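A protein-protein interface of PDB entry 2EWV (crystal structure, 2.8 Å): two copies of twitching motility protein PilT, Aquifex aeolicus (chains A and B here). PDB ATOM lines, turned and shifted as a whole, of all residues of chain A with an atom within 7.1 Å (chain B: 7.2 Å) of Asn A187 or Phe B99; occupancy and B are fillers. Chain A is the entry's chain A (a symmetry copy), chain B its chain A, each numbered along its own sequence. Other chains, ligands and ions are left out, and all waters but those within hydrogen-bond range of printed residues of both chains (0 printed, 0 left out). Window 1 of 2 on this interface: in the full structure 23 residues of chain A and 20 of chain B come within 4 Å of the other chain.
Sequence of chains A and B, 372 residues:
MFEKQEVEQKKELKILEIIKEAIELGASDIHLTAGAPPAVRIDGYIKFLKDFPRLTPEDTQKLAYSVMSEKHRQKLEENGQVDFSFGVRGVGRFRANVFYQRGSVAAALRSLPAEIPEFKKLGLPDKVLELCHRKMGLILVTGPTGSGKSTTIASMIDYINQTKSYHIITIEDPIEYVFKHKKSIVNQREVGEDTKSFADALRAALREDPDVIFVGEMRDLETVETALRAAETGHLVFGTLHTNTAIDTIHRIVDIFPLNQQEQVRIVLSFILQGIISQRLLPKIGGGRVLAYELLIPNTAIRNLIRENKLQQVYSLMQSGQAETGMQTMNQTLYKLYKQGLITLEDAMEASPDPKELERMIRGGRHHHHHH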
ATOM      1  N   HIS A 167     -13.079  10.248  18.393  1.00  0.00           N
ATOM      2  CA  HIS A 167     -13.762  11.529  18.551  1.00  0.00           C
ATOM      3  C   HIS A 167     -14.120  11.818  17.081  1.00  0.00           C
ATOM      4  O   HIS A 167     -13.242  12.176  16.299  1.00  0.00           O
ATOM      5  CB  HIS A 167     -12.821  12.633  19.063  1.00  0.00           C
ATOM      6  CG  HIS A 167     -13.325  14.024  18.790  1.00  0.00           C
ATOM      7  ND1 HIS A 167     -12.483  15.105  18.635  1.00  0.00           N
ATOM      8  CD2 HIS A 167     -14.579  14.495  18.586  1.00  0.00           C
ATOM      9  CE1 HIS A 167     -13.194  16.180  18.341  1.00  0.00           C
ATOM     10  NE2 HIS A 167     -14.468  15.836  18.306  1.00  0.00           N
ATOM     11  N   ILE A 168     -15.376  11.633  16.686  1.00  0.00           N
ATOM     12  CA  ILE A 168     -15.739  11.886  15.299  1.00  0.00           C
ATOM     13  C   ILE A 168     -16.358  13.248  15.177  1.00  0.00           C
ATOM     14  O   ILE A 168     -17.231  13.601  15.947  1.00  0.00           O
ATOM     15  CB  ILE A 168     -16.714  10.828  14.769  1.00  0.00           C
ATOM     16  CG1 ILE A 168     -16.110   9.449  14.993  1.00  0.00           C
ATOM     17  CG2 ILE A 168     -16.972  11.047  13.277  1.00  0.00           C
ATOM     18  CD1 ILE A 168     -17.010   8.346  14.649  1.00  0.00           C
ATOM     19  N   ILE A 169     -15.898  14.013  14.196  1.00  0.00           N
ATOM     20  CA  ILE A 169     -16.389  15.372  13.972  1.00  0.00           C
ATOM     21  C   ILE A 169     -17.066  15.547  12.579  1.00  0.00           C
ATOM     22  O   ILE A 169     -16.478  15.247  11.535  1.00  0.00           O
ATOM     23  CB  ILE A 169     -15.197  16.364  14.169  1.00  0.00           C
ATOM     24  CG1 ILE A 169     -15.704  17.774  14.439  1.00  0.00           C
ATOM     25  CG2 ILE A 169     -14.262  16.303  12.965  1.00  0.00           C
ATOM     26  CD1 ILE A 169     -14.609  18.663  14.936  1.00  0.00           C
ATOM     27  N   THR A 170     -18.313  16.008  12.566  1.00  0.00           N
ATOM     28  CA  THR A 170     -19.014  16.198  11.302  1.00  0.00           C
ATOM     29  C   THR A 170     -19.431  17.649  11.083  1.00  0.00           C
ATOM     30  O   THR A 170     -19.984  18.282  11.979  1.00  0.00           O
ATOM     31  CB  THR A 170     -20.296  15.313  11.204  1.00  0.00           C
ATOM     32  OG1 THR A 170     -21.266  15.767  12.152  1.00  0.00           O
ATOM     33  CG2 THR A 170     -19.981  13.853  11.479  1.00  0.00           C
ATOM     34  N   ILE A 171     -19.156  18.170   9.888  1.00  0.00           N
ATOM     35  CA  ILE A 171     -19.522  19.548   9.510  1.00  0.00           C
ATOM     36  C   ILE A 171     -20.672  19.432   8.497  1.00  0.00           C
ATOM     37  O   ILE A 171     -20.439  19.169   7.313  1.00  0.00           O
ATOM     38  CB  ILE A 171     -18.326  20.312   8.834  1.00  0.00           C
ATOM     39  CG1 ILE A 171     -17.025  20.106   9.620  1.00  0.00           C
ATOM     40  CG2 ILE A 171     -18.626  21.801   8.797  1.00  0.00           C
ATOM     41  CD1 ILE A 171     -15.796  20.462   8.833  1.00  0.00           C
ATOM     42  N   GLU A 172     -21.905  19.631   8.961  1.00  0.00           N
ATOM     43  CA  GLU A 172     -23.072  19.495   8.091  1.00  0.00           C
ATOM     44  C   GLU A 172     -23.886  20.753   7.742  1.00  0.00           C
ATOM     45  O   GLU A 172     -23.804  21.779   8.423  1.00  0.00           O
ATOM     46  CB  GLU A 172     -24.021  18.469   8.696  1.00  0.00           C
ATOM     47  CG  GLU A 172     -23.485  17.076   8.789  1.00  0.00           C
ATOM     48  CD  GLU A 172     -24.554  16.132   9.270  1.00  0.00           C
ATOM     49  OE1 GLU A 172     -25.606  16.041   8.604  1.00  0.00           O
ATOM     50  OE2 GLU A 172     -24.354  15.490  10.320  1.00  0.00           O
ATOM     51  N   PHE A 179     -26.313  11.763  15.865  1.00  0.00           N
ATOM     52  CA  PHE A 179     -25.604  10.623  16.438  1.00  0.00           C
ATOM     53  C   PHE A 179     -25.532  10.496  17.976  1.00  0.00           C
ATOM     54  O   PHE A 179     -25.223  11.448  18.704  1.00  0.00           O
ATOM     55  CB  PHE A 179     -24.173  10.551  15.877  1.00  0.00           C
ATOM     56  CG  PHE A 179     -24.070  10.566  14.355  1.00  0.00           C
ATOM     57  CD1 PHE A 179     -24.065  11.766  13.650  1.00  0.00           C
ATOM     58  CD2 PHE A 179     -23.846   9.388  13.648  1.00  0.00           C
ATOM     59  CE1 PHE A 179     -23.822  11.794  12.270  1.00  0.00           C
ATOM     60  CE2 PHE A 179     -23.603   9.408  12.271  1.00  0.00           C
ATOM     61  CZ  PHE A 179     -23.592  10.618  11.585  1.00  0.00           C
ATOM     62  N   HIS A 181     -23.871   9.171  21.337  1.00  0.00           N
ATOM     63  CA  HIS A 181     -22.510   8.874  21.790  1.00  0.00           C
ATOM     64  C   HIS A 181     -22.481   7.380  22.115  1.00  0.00           C
ATOM     65  O   HIS A 181     -23.221   6.922  22.988  1.00  0.00           O
ATOM     66  CB  HIS A 181     -22.162   9.639  23.077  1.00  0.00           C
ATOM     67  CG  HIS A 181     -22.042  11.123  22.908  1.00  0.00           C
ATOM     68  ND1 HIS A 181     -20.957  11.720  22.303  1.00  0.00           N
ATOM     69  CD2 HIS A 181     -22.851  12.132  23.313  1.00  0.00           C
ATOM     70  CE1 HIS A 181     -21.100  13.032  22.347  1.00  0.00           C
ATOM     71  NE2 HIS A 181     -22.239  13.309  22.956  1.00  0.00           N
ATOM     72  N   ILE A 185     -17.081   9.607  21.005  1.00  0.00           N
ATOM     73  CA  ILE A 185     -17.693  10.912  21.172  1.00  0.00           C
ATOM     74  C   ILE A 185     -17.887  11.654  19.820  1.00  0.00           C
ATOM     75  O   ILE A 185     -16.924  12.029  19.158  1.00  0.00           O
ATOM     76  CB  ILE A 185     -16.822  11.738  22.186  1.00  0.00           C
ATOM     77  CG1 ILE A 185     -17.269  13.197  22.247  1.00  0.00           C
ATOM     78  CG2 ILE A 185     -15.354  11.647  21.809  1.00  0.00           C
ATOM     79  CD1 ILE A 185     -16.310  14.091  23.037  1.00  0.00           C
ATOM     80  N   VAL A 186     -19.145  11.844  19.416  1.00  0.00           N
ATOM     81  CA  VAL A 186     -19.494  12.538  18.165  1.00  0.00           C
ATOM     82  C   VAL A 186     -19.819  14.016  18.419  1.00  0.00           C
ATOM     83  O   VAL A 186     -20.480  14.348  19.410  1.00  0.00           O
ATOM     84  CB  VAL A 186     -20.732  11.909  17.492  1.00  0.00           C
ATOM     85  CG1 VAL A 186     -21.069  12.673  16.210  1.00  0.00           C
ATOM     86  CG2 VAL A 186     -20.486  10.450  17.218  1.00  0.00           C
ATOM     87  N   ASN A 187     -19.353  14.887  17.518  1.00  0.00           N
ATOM     88  CA  ASN A 187     -19.557  16.344  17.605  1.00  0.00           C
ATOM     89  C   ASN A 187     -20.118  16.780  16.275  1.00  0.00           C
ATOM     90  O   ASN A 187     -19.457  16.630  15.254  1.00  0.00           O
ATOM     91  CB  ASN A 187     -18.228  17.088  17.838  1.00  0.00           C
ATOM     92  CG  ASN A 187     -17.702  16.943  19.263  1.00  0.00           C
ATOM     93  OD1 ASN A 187     -16.626  17.448  19.599  1.00  0.00           O
ATOM     94  ND2 ASN A 187     -18.456  16.253  20.103  1.00  0.00           N
ATOM     95  N   GLN A 188     -21.319  17.349  16.287  1.00  0.00           N
ATOM     96  CA  GLN A 188     -21.981  17.766  15.044  1.00  0.00           C
ATOM     97  C   GLN A 188     -22.335  19.254  14.875  1.00  0.00           C
ATOM     98  O   GLN A 188     -23.341  19.715  15.425  1.00  0.00           O
ATOM     99  CB  GLN A 188     -23.245  16.933  14.859  1.00  0.00           C
ATOM    100  CG  GLN A 188     -22.999  15.488  14.481  1.00  0.00           C
ATOM    101  CD  GLN A 188     -24.287  14.746  14.366  1.00  0.00           C
ATOM    102  OE1 GLN A 188     -24.870  14.364  15.370  1.00  0.00           O
ATOM    103  NE2 GLN A 188     -24.768  14.565  13.141  1.00  0.00           N
ATOM    104  N   ARG A 189     -21.539  19.971  14.068  1.00  0.00           N
ATOM    105  CA  ARG A 189     -21.717  21.414  13.811  1.00  0.00           C
ATOM    106  C   ARG A 189     -22.484  21.802  12.532  1.00  0.00           C
ATOM    107  O   ARG A 189     -22.042  21.484  11.409  1.00  0.00           O
ATOM    108  CB  ARG A 189     -20.353  22.106  13.767  1.00  0.00           C
ATOM    109  CG  ARG A 189     -19.351  21.584  14.756  1.00  0.00           C
ATOM    110  CD  ARG A 189     -18.115  22.419  14.680  1.00  0.00           C
ATOM    111  NE  ARG A 189     -18.358  23.747  15.237  1.00  0.00           N
ATOM    112  CZ  ARG A 189     -17.629  24.827  14.966  1.00  0.00           C
ATOM    113  NH1 ARG A 189     -17.930  25.987  15.535  1.00  0.00           N
ATOM    114  NH2 ARG A 189     -16.617  24.755  14.110  1.00  0.00           N
ATOM    115  N   ASP A 194     -23.907  26.953  13.782  1.00  0.00           N
ATOM    116  CA  ASP A 194     -22.792  26.707  14.714  1.00  0.00           C
ATOM    117  C   ASP A 194     -21.470  27.330  14.290  1.00  0.00           C
ATOM    118  O   ASP A 194     -20.592  27.593  15.102  1.00  0.00           O
ATOM    119  CB  ASP A 194     -22.592  25.203  14.882  1.00  0.00           C
ATOM    120  CG  ASP A 194     -23.789  24.535  15.507  1.00  0.00           C
ATOM    121  OD1 ASP A 194     -24.332  23.585  14.899  1.00  0.00           O
ATOM    122  OD2 ASP A 194     -24.185  24.978  16.611  1.00  0.00           O
ATOM    123  N   THR A 195     -21.336  27.531  12.998  1.00  0.00           N
ATOM    124  CA  THR A 195     -20.155  28.125  12.416  1.00  0.00           C
ATOM    125  C   THR A 195     -20.764  28.837  11.242  1.00  0.00           C
ATOM    126  O   THR A 195     -21.984  28.965  11.166  1.00  0.00           O
ATOM    127  CB  THR A 195     -19.212  27.063  11.878  1.00  0.00           C
ATOM    128  OG1 THR A 195     -19.770  25.769  12.133  1.00  0.00           O
ATOM    129  CG2 THR A 195     -17.850  27.185  12.523  1.00  0.00           C
ATOM    130  N   ALA A 204     -10.766  24.495  11.750  1.00  0.00           N
ATOM    131  CA  ALA A 204     -10.722  24.285  13.192  1.00  0.00           C
ATOM    132  C   ALA A 204     -10.785  22.795  13.488  1.00  0.00           C
ATOM    133  O   ALA A 204     -10.177  22.334  14.443  1.00  0.00           O
ATOM    134  CB  ALA A 204     -11.877  25.003  13.879  1.00  0.00           C
ATOM    135  N   GLU A 208      -8.772  20.239  16.722  1.00  0.00           N
ATOM    136  CA  GLU A 208      -9.762  19.848  17.739  1.00  0.00           C
ATOM    137  C   GLU A 208      -9.598  18.373  18.072  1.00  0.00           C
ATOM    138  O   GLU A 208     -10.442  17.775  18.729  1.00  0.00           O
ATOM    139  CB  GLU A 208     -11.190  20.121  17.270  1.00  0.00           C
ATOM    140  CG  GLU A 208     -11.480  21.603  17.134  1.00  0.00           C
ATOM    141  CD  GLU A 208     -12.909  21.900  16.760  1.00  0.00           C
ATOM    142  OE1 GLU A 208     -13.163  23.014  16.252  1.00  0.00           O
ATOM    143  OE2 GLU A 208     -13.774  21.026  16.986  1.00  0.00           O
ATOM    144  N   PRO A 210      -9.927  15.693  16.256  1.00  0.00           N
ATOM    145  CA  PRO A 210     -10.900  14.710  15.774  1.00  0.00           C
ATOM    146  C   PRO A 210     -10.210  13.547  15.056  1.00  0.00           C
ATOM    147  O   PRO A 210      -9.194  13.738  14.376  1.00  0.00           O
ATOM    148  CB  PRO A 210     -11.774  15.534  14.838  1.00  0.00           C
ATOM    149  CG  PRO A 210     -10.783  16.433  14.195  1.00  0.00           C
ATOM    150  CD  PRO A 210      -9.961  16.897  15.400  1.00  0.00           C
ATOM    151  N   HIS B  31     -11.855  15.639  26.394  1.00  0.00           N
ATOM    152  CA  HIS B  31     -12.955  16.228  25.626  1.00  0.00           C
ATOM    153  C   HIS B  31     -14.245  16.339  26.433  1.00  0.00           C
ATOM    154  O   HIS B  31     -14.673  15.385  27.080  1.00  0.00           O
ATOM    155  CB  HIS B  31     -13.224  15.402  24.359  1.00  0.00           C
ATOM    156  CG  HIS B  31     -12.113  15.447  23.347  1.00  0.00           C
ATOM    157  ND1 HIS B  31     -12.058  16.386  22.339  1.00  0.00           N
ATOM    158  CD2 HIS B  31     -11.017  14.666  23.191  1.00  0.00           C
ATOM    159  CE1 HIS B  31     -10.979  16.181  21.606  1.00  0.00           C
ATOM    160  NE2 HIS B  31     -10.329  15.142  22.101  1.00  0.00           N
ATOM    161  N   LEU B  32     -14.864  17.512  26.391  1.00  0.00           N
ATOM    162  CA  LEU B  32     -16.108  17.745  27.109  1.00  0.00           C
ATOM    163  C   LEU B  32     -17.178  18.013  26.062  1.00  0.00           C
ATOM    164  O   LEU B  32     -17.178  19.047  25.395  1.00  0.00           O
ATOM    165  CB  LEU B  32     -15.955  18.948  28.048  1.00  0.00           C
ATOM    166  CG  LEU B  32     -14.676  19.004  28.901  1.00  0.00           C
ATOM    167  CD1 LEU B  32     -14.543  20.383  29.520  1.00  0.00           C
ATOM    168  CD2 LEU B  32     -14.694  17.916  29.975  1.00  0.00           C
ATOM    169  N   THR B  33     -18.086  17.064  25.899  1.00  0.00           N
ATOM    170  CA  THR B  33     -19.136  17.227  24.915  1.00  0.00           C
ATOM    171  C   THR B  33     -20.453  17.443  25.656  1.00  0.00           C
ATOM    172  O   THR B  33     -20.434  17.855  26.808  1.00  0.00           O
ATOM    173  CB  THR B  33     -19.185  16.002  23.987  1.00  0.00           C
ATOM    174  OG1 THR B  33     -20.074  16.256  22.894  1.00  0.00           O
ATOM    175  CG2 THR B  33     -19.634  14.781  24.762  1.00  0.00           C
ATOM    176  N   ALA B  34     -21.590  17.169  25.030  1.00  0.00           N
ATOM    177  CA  ALA B  34     -22.861  17.412  25.702  1.00  0.00           C
ATOM    178  C   ALA B  34     -23.607  16.187  26.198  1.00  0.00           C
ATOM    179  O   ALA B  34     -24.215  16.218  27.267  1.00  0.00           O
ATOM    180  CB  ALA B  34     -23.764  18.232  24.802  1.00  0.00           C
ATOM    181  N   LEU B  76     -16.357  33.535  20.812  1.00  0.00           N
ATOM    182  CA  LEU B  76     -17.074  32.283  20.607  1.00  0.00           C
ATOM    183  C   LEU B  76     -18.451  32.599  20.057  1.00  0.00           C
ATOM    184  O   LEU B  76     -19.215  31.700  19.708  1.00  0.00           O
ATOM    185  CB  LEU B  76     -17.228  31.517  21.920  1.00  0.00           C
ATOM    186  CG  LEU B  76     -17.886  30.144  21.753  1.00  0.00           C
ATOM    187  CD1 LEU B  76     -16.900  29.191  21.095  1.00  0.00           C
ATOM    188  CD2 LEU B  76     -18.328  29.611  23.101  1.00  0.00           C
ATOM    189  N   ASN B  79     -17.877  33.928  15.732  1.00  0.00           N
ATOM    190  CA  ASN B  79     -17.803  32.643  15.042  1.00  0.00           C
ATOM    191  C   ASN B  79     -17.975  31.619  16.165  1.00  0.00           C
ATOM    192  O   ASN B  79     -17.574  31.870  17.299  1.00  0.00           O
ATOM    193  CB  ASN B  79     -16.466  32.462  14.286  1.00  0.00           C
ATOM    194  CG  ASN B  79     -15.327  33.316  14.851  1.00  0.00           C
ATOM    195  OD1 ASN B  79     -15.469  34.532  15.019  1.00  0.00           O
ATOM    196  ND2 ASN B  79     -14.181  32.678  15.122  1.00  0.00           N
ATOM    197  N   GLY B  80     -18.597  30.487  15.871  1.00  0.00           N
ATOM    198  CA  GLY B  80     -18.822  29.503  16.914  1.00  0.00           C
ATOM    199  C   GLY B  80     -17.603  28.761  17.418  1.00  0.00           C
ATOM    200  O   GLY B  80     -17.646  27.539  17.537  1.00  0.00           O
ATOM    201  N   GLN B  81     -16.532  29.484  17.742  1.00  0.00           N
ATOM    202  CA  GLN B  81     -15.306  28.844  18.211  1.00  0.00           C
ATOM    203  C   GLN B  81     -14.212  29.803  18.666  1.00  0.00           C
ATOM    204  O   GLN B  81     -14.167  30.958  18.245  1.00  0.00           O
ATOM    205  CB  GLN B  81     -14.725  27.989  17.094  1.00  0.00           C
ATOM    206  CG  GLN B  81     -14.320  28.815  15.884  1.00  0.00           C
ATOM    207  CD  GLN B  81     -15.025  28.381  14.623  1.00  0.00           C
ATOM    208  OE1 GLN B  81     -15.070  29.116  13.637  1.00  0.00           O
ATOM    209  NE2 GLN B  81     -15.577  27.177  14.641  1.00  0.00           N
ATOM    210  N   VAL B  82     -13.319  29.295  19.514  1.00  0.00           N
ATOM    211  CA  VAL B  82     -12.170  30.051  20.021  1.00  0.00           C
ATOM    212  C   VAL B  82     -10.998  29.123  20.226  1.00  0.00           C
ATOM    213  O   VAL B  82     -11.156  28.018  20.728  1.00  0.00           O
ATOM    214  CB  VAL B  82     -12.411  30.711  21.396  1.00  0.00           C
ATOM    215  CG1 VAL B  82     -12.945  32.109  21.214  1.00  0.00           C
ATOM    216  CG2 VAL B  82     -13.340  29.853  22.241  1.00  0.00           C
ATOM    217  N   ASN B  97     -10.029  24.711  22.771  1.00  0.00           N
ATOM    218  CA  ASN B  97     -10.700  25.065  21.521  1.00  0.00           C
ATOM    219  C   ASN B  97     -12.192  24.808  21.707  1.00  0.00           C
ATOM    220  O   ASN B  97     -12.691  23.742  21.364  1.00  0.00           O
ATOM    221  CB  ASN B  97     -10.193  24.227  20.346  1.00  0.00           C
ATOM    222  CG  ASN B  97     -10.825  24.646  19.021  1.00  0.00           C
ATOM    223  OD1 ASN B  97     -12.047  24.777  18.911  1.00  0.00           O
ATOM    224  ND2 ASN B  97      -9.991  24.858  18.007  1.00  0.00           N
ATOM    225  N   VAL B  98     -12.896  25.786  22.260  1.00  0.00           N
ATOM    226  CA  VAL B  98     -14.321  25.659  22.496  1.00  0.00           C
ATOM    227  C   VAL B  98     -15.025  26.030  21.212  1.00  0.00           C
ATOM    228  O   VAL B  98     -14.534  26.854  20.450  1.00  0.00           O
ATOM    229  CB  VAL B  98     -14.777  26.604  23.625  1.00  0.00           C
ATOM    230  CG1 VAL B  98     -16.176  26.228  24.090  1.00  0.00           C
ATOM    231  CG2 VAL B  98     -13.783  26.542  24.783  1.00  0.00           C
ATOM    232  N   PHE B  99     -16.177  25.416  20.972  1.00  0.00           N
ATOM    233  CA  PHE B  99     -16.950  25.682  19.755  1.00  0.00           C
ATOM    234  C   PHE B  99     -18.392  25.314  19.933  1.00  0.00           C
ATOM    235  O   PHE B  99     -18.705  24.456  20.753  1.00  0.00           O
ATOM    236  CB  PHE B  99     -16.410  24.850  18.587  1.00  0.00           C
ATOM    237  CG  PHE B  99     -16.209  23.401  18.936  1.00  0.00           C
ATOM    238  CD1 PHE B  99     -15.076  23.002  19.636  1.00  0.00           C
ATOM    239  CD2 PHE B  99     -17.164  22.446  18.621  1.00  0.00           C
ATOM    240  CE1 PHE B  99     -14.888  21.679  20.022  1.00  0.00           C
ATOM    241  CE2 PHE B  99     -16.987  21.110  19.005  1.00  0.00           C
ATOM    242  CZ  PHE B  99     -15.842  20.727  19.709  1.00  0.00           C
ATOM    243  N   TYR B 100     -19.273  25.945  19.156  1.00  0.00           N
ATOM    244  CA  TYR B 100     -20.697  25.592  19.218  1.00  0.00           C
ATOM    245  C   TYR B 100     -20.793  24.316  18.432  1.00  0.00           C
ATOM    246  O   TYR B 100     -20.596  24.281  17.213  1.00  0.00           O
ATOM    247  CB  TYR B 100     -21.575  26.671  18.607  1.00  0.00           C
ATOM    248  CG  TYR B 100     -21.886  27.802  19.544  1.00  0.00           C
ATOM    249  CD1 TYR B 100     -22.229  29.062  19.043  1.00  0.00           C
ATOM    250  CD2 TYR B 100     -21.816  27.634  20.931  1.00  0.00           C
ATOM    251  CE1 TYR B 100     -22.484  30.130  19.904  1.00  0.00           C
ATOM    252  CE2 TYR B 100     -22.071  28.692  21.795  1.00  0.00           C
ATOM    253  CZ  TYR B 100     -22.398  29.932  21.280  1.00  0.00           C
ATOM    254  OH  TYR B 100     -22.609  30.977  22.148  1.00  0.00           O
ATOM    255  N   GLN B 101     -21.109  23.257  19.146  1.00  0.00           N
ATOM    256  CA  GLN B 101     -21.126  21.965  18.523  1.00  0.00           C
ATOM    257  C   GLN B 101     -22.421  21.616  17.842  1.00  0.00           C
ATOM    258  O   GLN B 101     -22.479  21.601  16.588  1.00  0.00           O
ATOM    259  CB  GLN B 101     -20.869  20.897  19.556  1.00  0.00           C
ATOM    260  CG  GLN B 101     -20.809  19.567  18.907  1.00  0.00           C
ATOM    261  CD  GLN B 101     -20.773  18.464  19.895  1.00  0.00           C
ATOM    262  OE1 GLN B 101     -19.944  18.459  20.811  1.00  0.00           O
ATOM    263  NE2 GLN B 101     -21.647  17.493  19.712  1.00  0.00           N
ATOM    264  N   ARG B 102     -23.452  21.251  18.616  1.00  0.00           N
ATOM    265  CA  ARG B 102     -24.696  20.901  17.938  1.00  0.00           C
ATOM    266  C   ARG B 102     -25.781  21.676  18.649  1.00  0.00           C
ATOM    267  O   ARG B 102     -26.798  21.176  19.144  1.00  0.00           O
ATOM    268  CB  ARG B 102     -24.866  19.403  18.046  1.00  0.00           C
ATOM    269  CG  ARG B 102     -26.236  18.817  17.994  1.00  0.00           C
ATOM    270  CD  ARG B 102     -26.083  17.330  17.689  1.00  0.00           C
ATOM    271  NE  ARG B 102     -26.197  16.389  18.814  1.00  0.00           N
ATOM    272  CZ  ARG B 102     -26.117  15.072  18.639  1.00  0.00           C
ATOM    273  NH1 ARG B 102     -25.917  14.647  17.405  1.00  0.00           N
ATOM    274  NH2 ARG B 102     -26.270  14.195  19.638  1.00  0.00           N
ATOM    275  N   SER B 104     -24.941  23.708  21.121  1.00  0.00           N
ATOM    276  CA  SER B 104     -24.597  23.793  22.547  1.00  0.00           C
ATOM    277  C   SER B 104     -23.269  24.540  22.843  1.00  0.00           C
ATOM    278  O   SER B 104     -23.210  25.790  22.825  1.00  0.00           O
ATOM    279  CB  SER B 104     -24.523  22.370  23.132  1.00  0.00           C
ATOM    280  OG  SER B 104     -24.514  22.390  24.539  1.00  0.00           O
ATOM    281  N   VAL B 105     -22.228  23.732  23.085  1.00  0.00           N
ATOM    282  CA  VAL B 105     -20.875  24.156  23.399  1.00  0.00           C
ATOM    283  C   VAL B 105     -20.081  22.901  23.689  1.00  0.00           C
ATOM    284  O   VAL B 105     -20.476  22.051  24.497  1.00  0.00           O
ATOM    285  CB  VAL B 105     -20.810  25.085  24.660  1.00  0.00           C
ATOM    286  CG1 VAL B 105     -20.754  26.524  24.218  1.00  0.00           C
ATOM    287  CG2 VAL B 105     -22.013  24.846  25.600  1.00  0.00           C
ATOM    288  N   ALA B 106     -18.938  22.802  23.036  1.00  0.00           N
ATOM    289  CA  ALA B 106     -18.081  21.663  23.224  1.00  0.00           C
ATOM    290  C   ALA B 106     -16.648  22.165  23.316  1.00  0.00           C
ATOM    291  O   ALA B 106     -16.253  23.138  22.655  1.00  0.00           O
ATOM    292  CB  ALA B 106     -18.248  20.696  22.072  1.00  0.00           C
ATOM    293  N   ALA B 107     -15.878  21.514  24.177  1.00  0.00           N
ATOM    294  CA  ALA B 107     -14.489  21.877  24.360  1.00  0.00           C
ATOM    295  C   ALA B 107     -13.527  20.697  24.194  1.00  0.00           C
ATOM    296  O   ALA B 107     -13.868  19.542  24.457  1.00  0.00           O
ATOM    297  CB  ALA B 107     -14.305  22.524  25.716  1.00  0.00           C
ATOM    298  N   ALA B 108     -12.322  21.023  23.742  1.00  0.00           N
ATOM    299  CA  ALA B 108     -11.255  20.055  23.518  1.00  0.00           C
ATOM    300  C   ALA B 108      -9.932  20.612  24.035  1.00  0.00           C
ATOM    301  O   ALA B 108      -9.213  21.294  23.306  1.00  0.00           O
ATOM    302  CB  ALA B 108     -11.130  19.747  22.036  1.00  0.00           C
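OG1 of Thr B33 lies within hydrogen-bond range of ND2 of Asn A187 (3.2 Å). The backbone carbonyl oxygen (O) of Gly B80 lies within hydrogen-bond range of the guanidinium group (NH1) of Arg A189, at 2.5 Å. NH2 of Arg A189 sits close to NE2 of Gln B81, at 2.7 Å. OD1 of Asn B97 lies close to OE1 of Glu A208 (3.4 Å). The guanidinium group of Arg A189 sits at hydrogen-bond distance from the backbone carbonyl oxygen of Tyr B100, 3.0 Å away. The side-chain amide nitrogen (NE2) of Gln B101 is in hydrogen-bond range of the backbone carbonyl oxygen (O) of Val A186. ND2 of Asn A187 lies within hydrogen-bond range of OE1 of Gln B101 (2.8 Å). NE2 of Gln B101 sits close to N of Gln A188, at 3.4 Å. The backbone NH (N) of Arg A189 sits close to the backbone carbonyl oxygen (O) of Gln B101, 3.1 Å away. The backbone carbonyl oxygen (O) of Phe A179 lies within hydrogen-bond range of the guanidinium group (NH2) of Arg B102 (3.1 Å). The side-chain amide oxygen (OE1) of Gln A188 lies close to the guanidinium group (NH1) of Arg B102. The backbone carbonyl oxygen (O) of Gln B101 lies close to the side-chain carboxylate (OD1) of Asp A194 (3.2 Å).
No position is printed for both chains.
Of the 20 printed residues of chain B, 10 touch a printed residue of chain A. Hydrophobic or aromatic side chains of chain B within 4 Å of the printed part of chain A: His B31, Phe B99, Tyr B100 and Ala B108. Among the printed residues, 25 pairs touch across the chains. Among the printed residues, no Asp or Glu carboxylate lies within 4 Å of a Lys or Arg side-chain nitrogen of the other chain.
Asn A187 touches just these residues of chain B: Thr B33, Phe B99 and Gln B101. Of the printed residues of chain A, His B31 touches His A167, Ile A185 and Glu A208. Of the printed residues of chain A, Thr B33 touches His A181, Ile A185, Val A186 and Asn A187. Of chain A, only Asn A187, Arg A189 and Glu A208 come within 4 Å of Phe B99. Of the printed residues of chain A, Ala B108 touches Glu A208 (3.9 Å). The nearest residue of chain B that does not touch Asn A187 is Ala B106 (4.4 Å). The nearest residue of chain A that does not touch Phe B99 is His A167 (5.3 Å). The nearest printed residue of chain B that does not touch Phe A179 is Gln B101 (7.1 Å).
NE2 of His A167 is in hydrogen-bond range of OD1 of Asn A187, 3.0 Å away. The backbone NH (N) of Asn A187 sits at hydrogen-bond distance from the backbone carbonyl oxygen (O) of Ile A168 (2.9 Å). ND1 of His A181 is in hydrogen-bond range of N of Val A186, 3.4 Å away.
His A167 touches His B31. Thr B33 touches His A181 (CG2 to CE1, 3.3 Å). CB of Thr B33 touches CD1 of Ile A185 (3.6 Å). Phe B99 touches Arg A189. Gly B80 touches Asp A194 (CA to O, 3.2 Å). Tyr B100 touches Asp A194. Gln B81 touches Thr A195 (NE2 to CG2, 3.1 Å). CE1 of His B31 touches O of Glu A208, 3.3 Å away.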
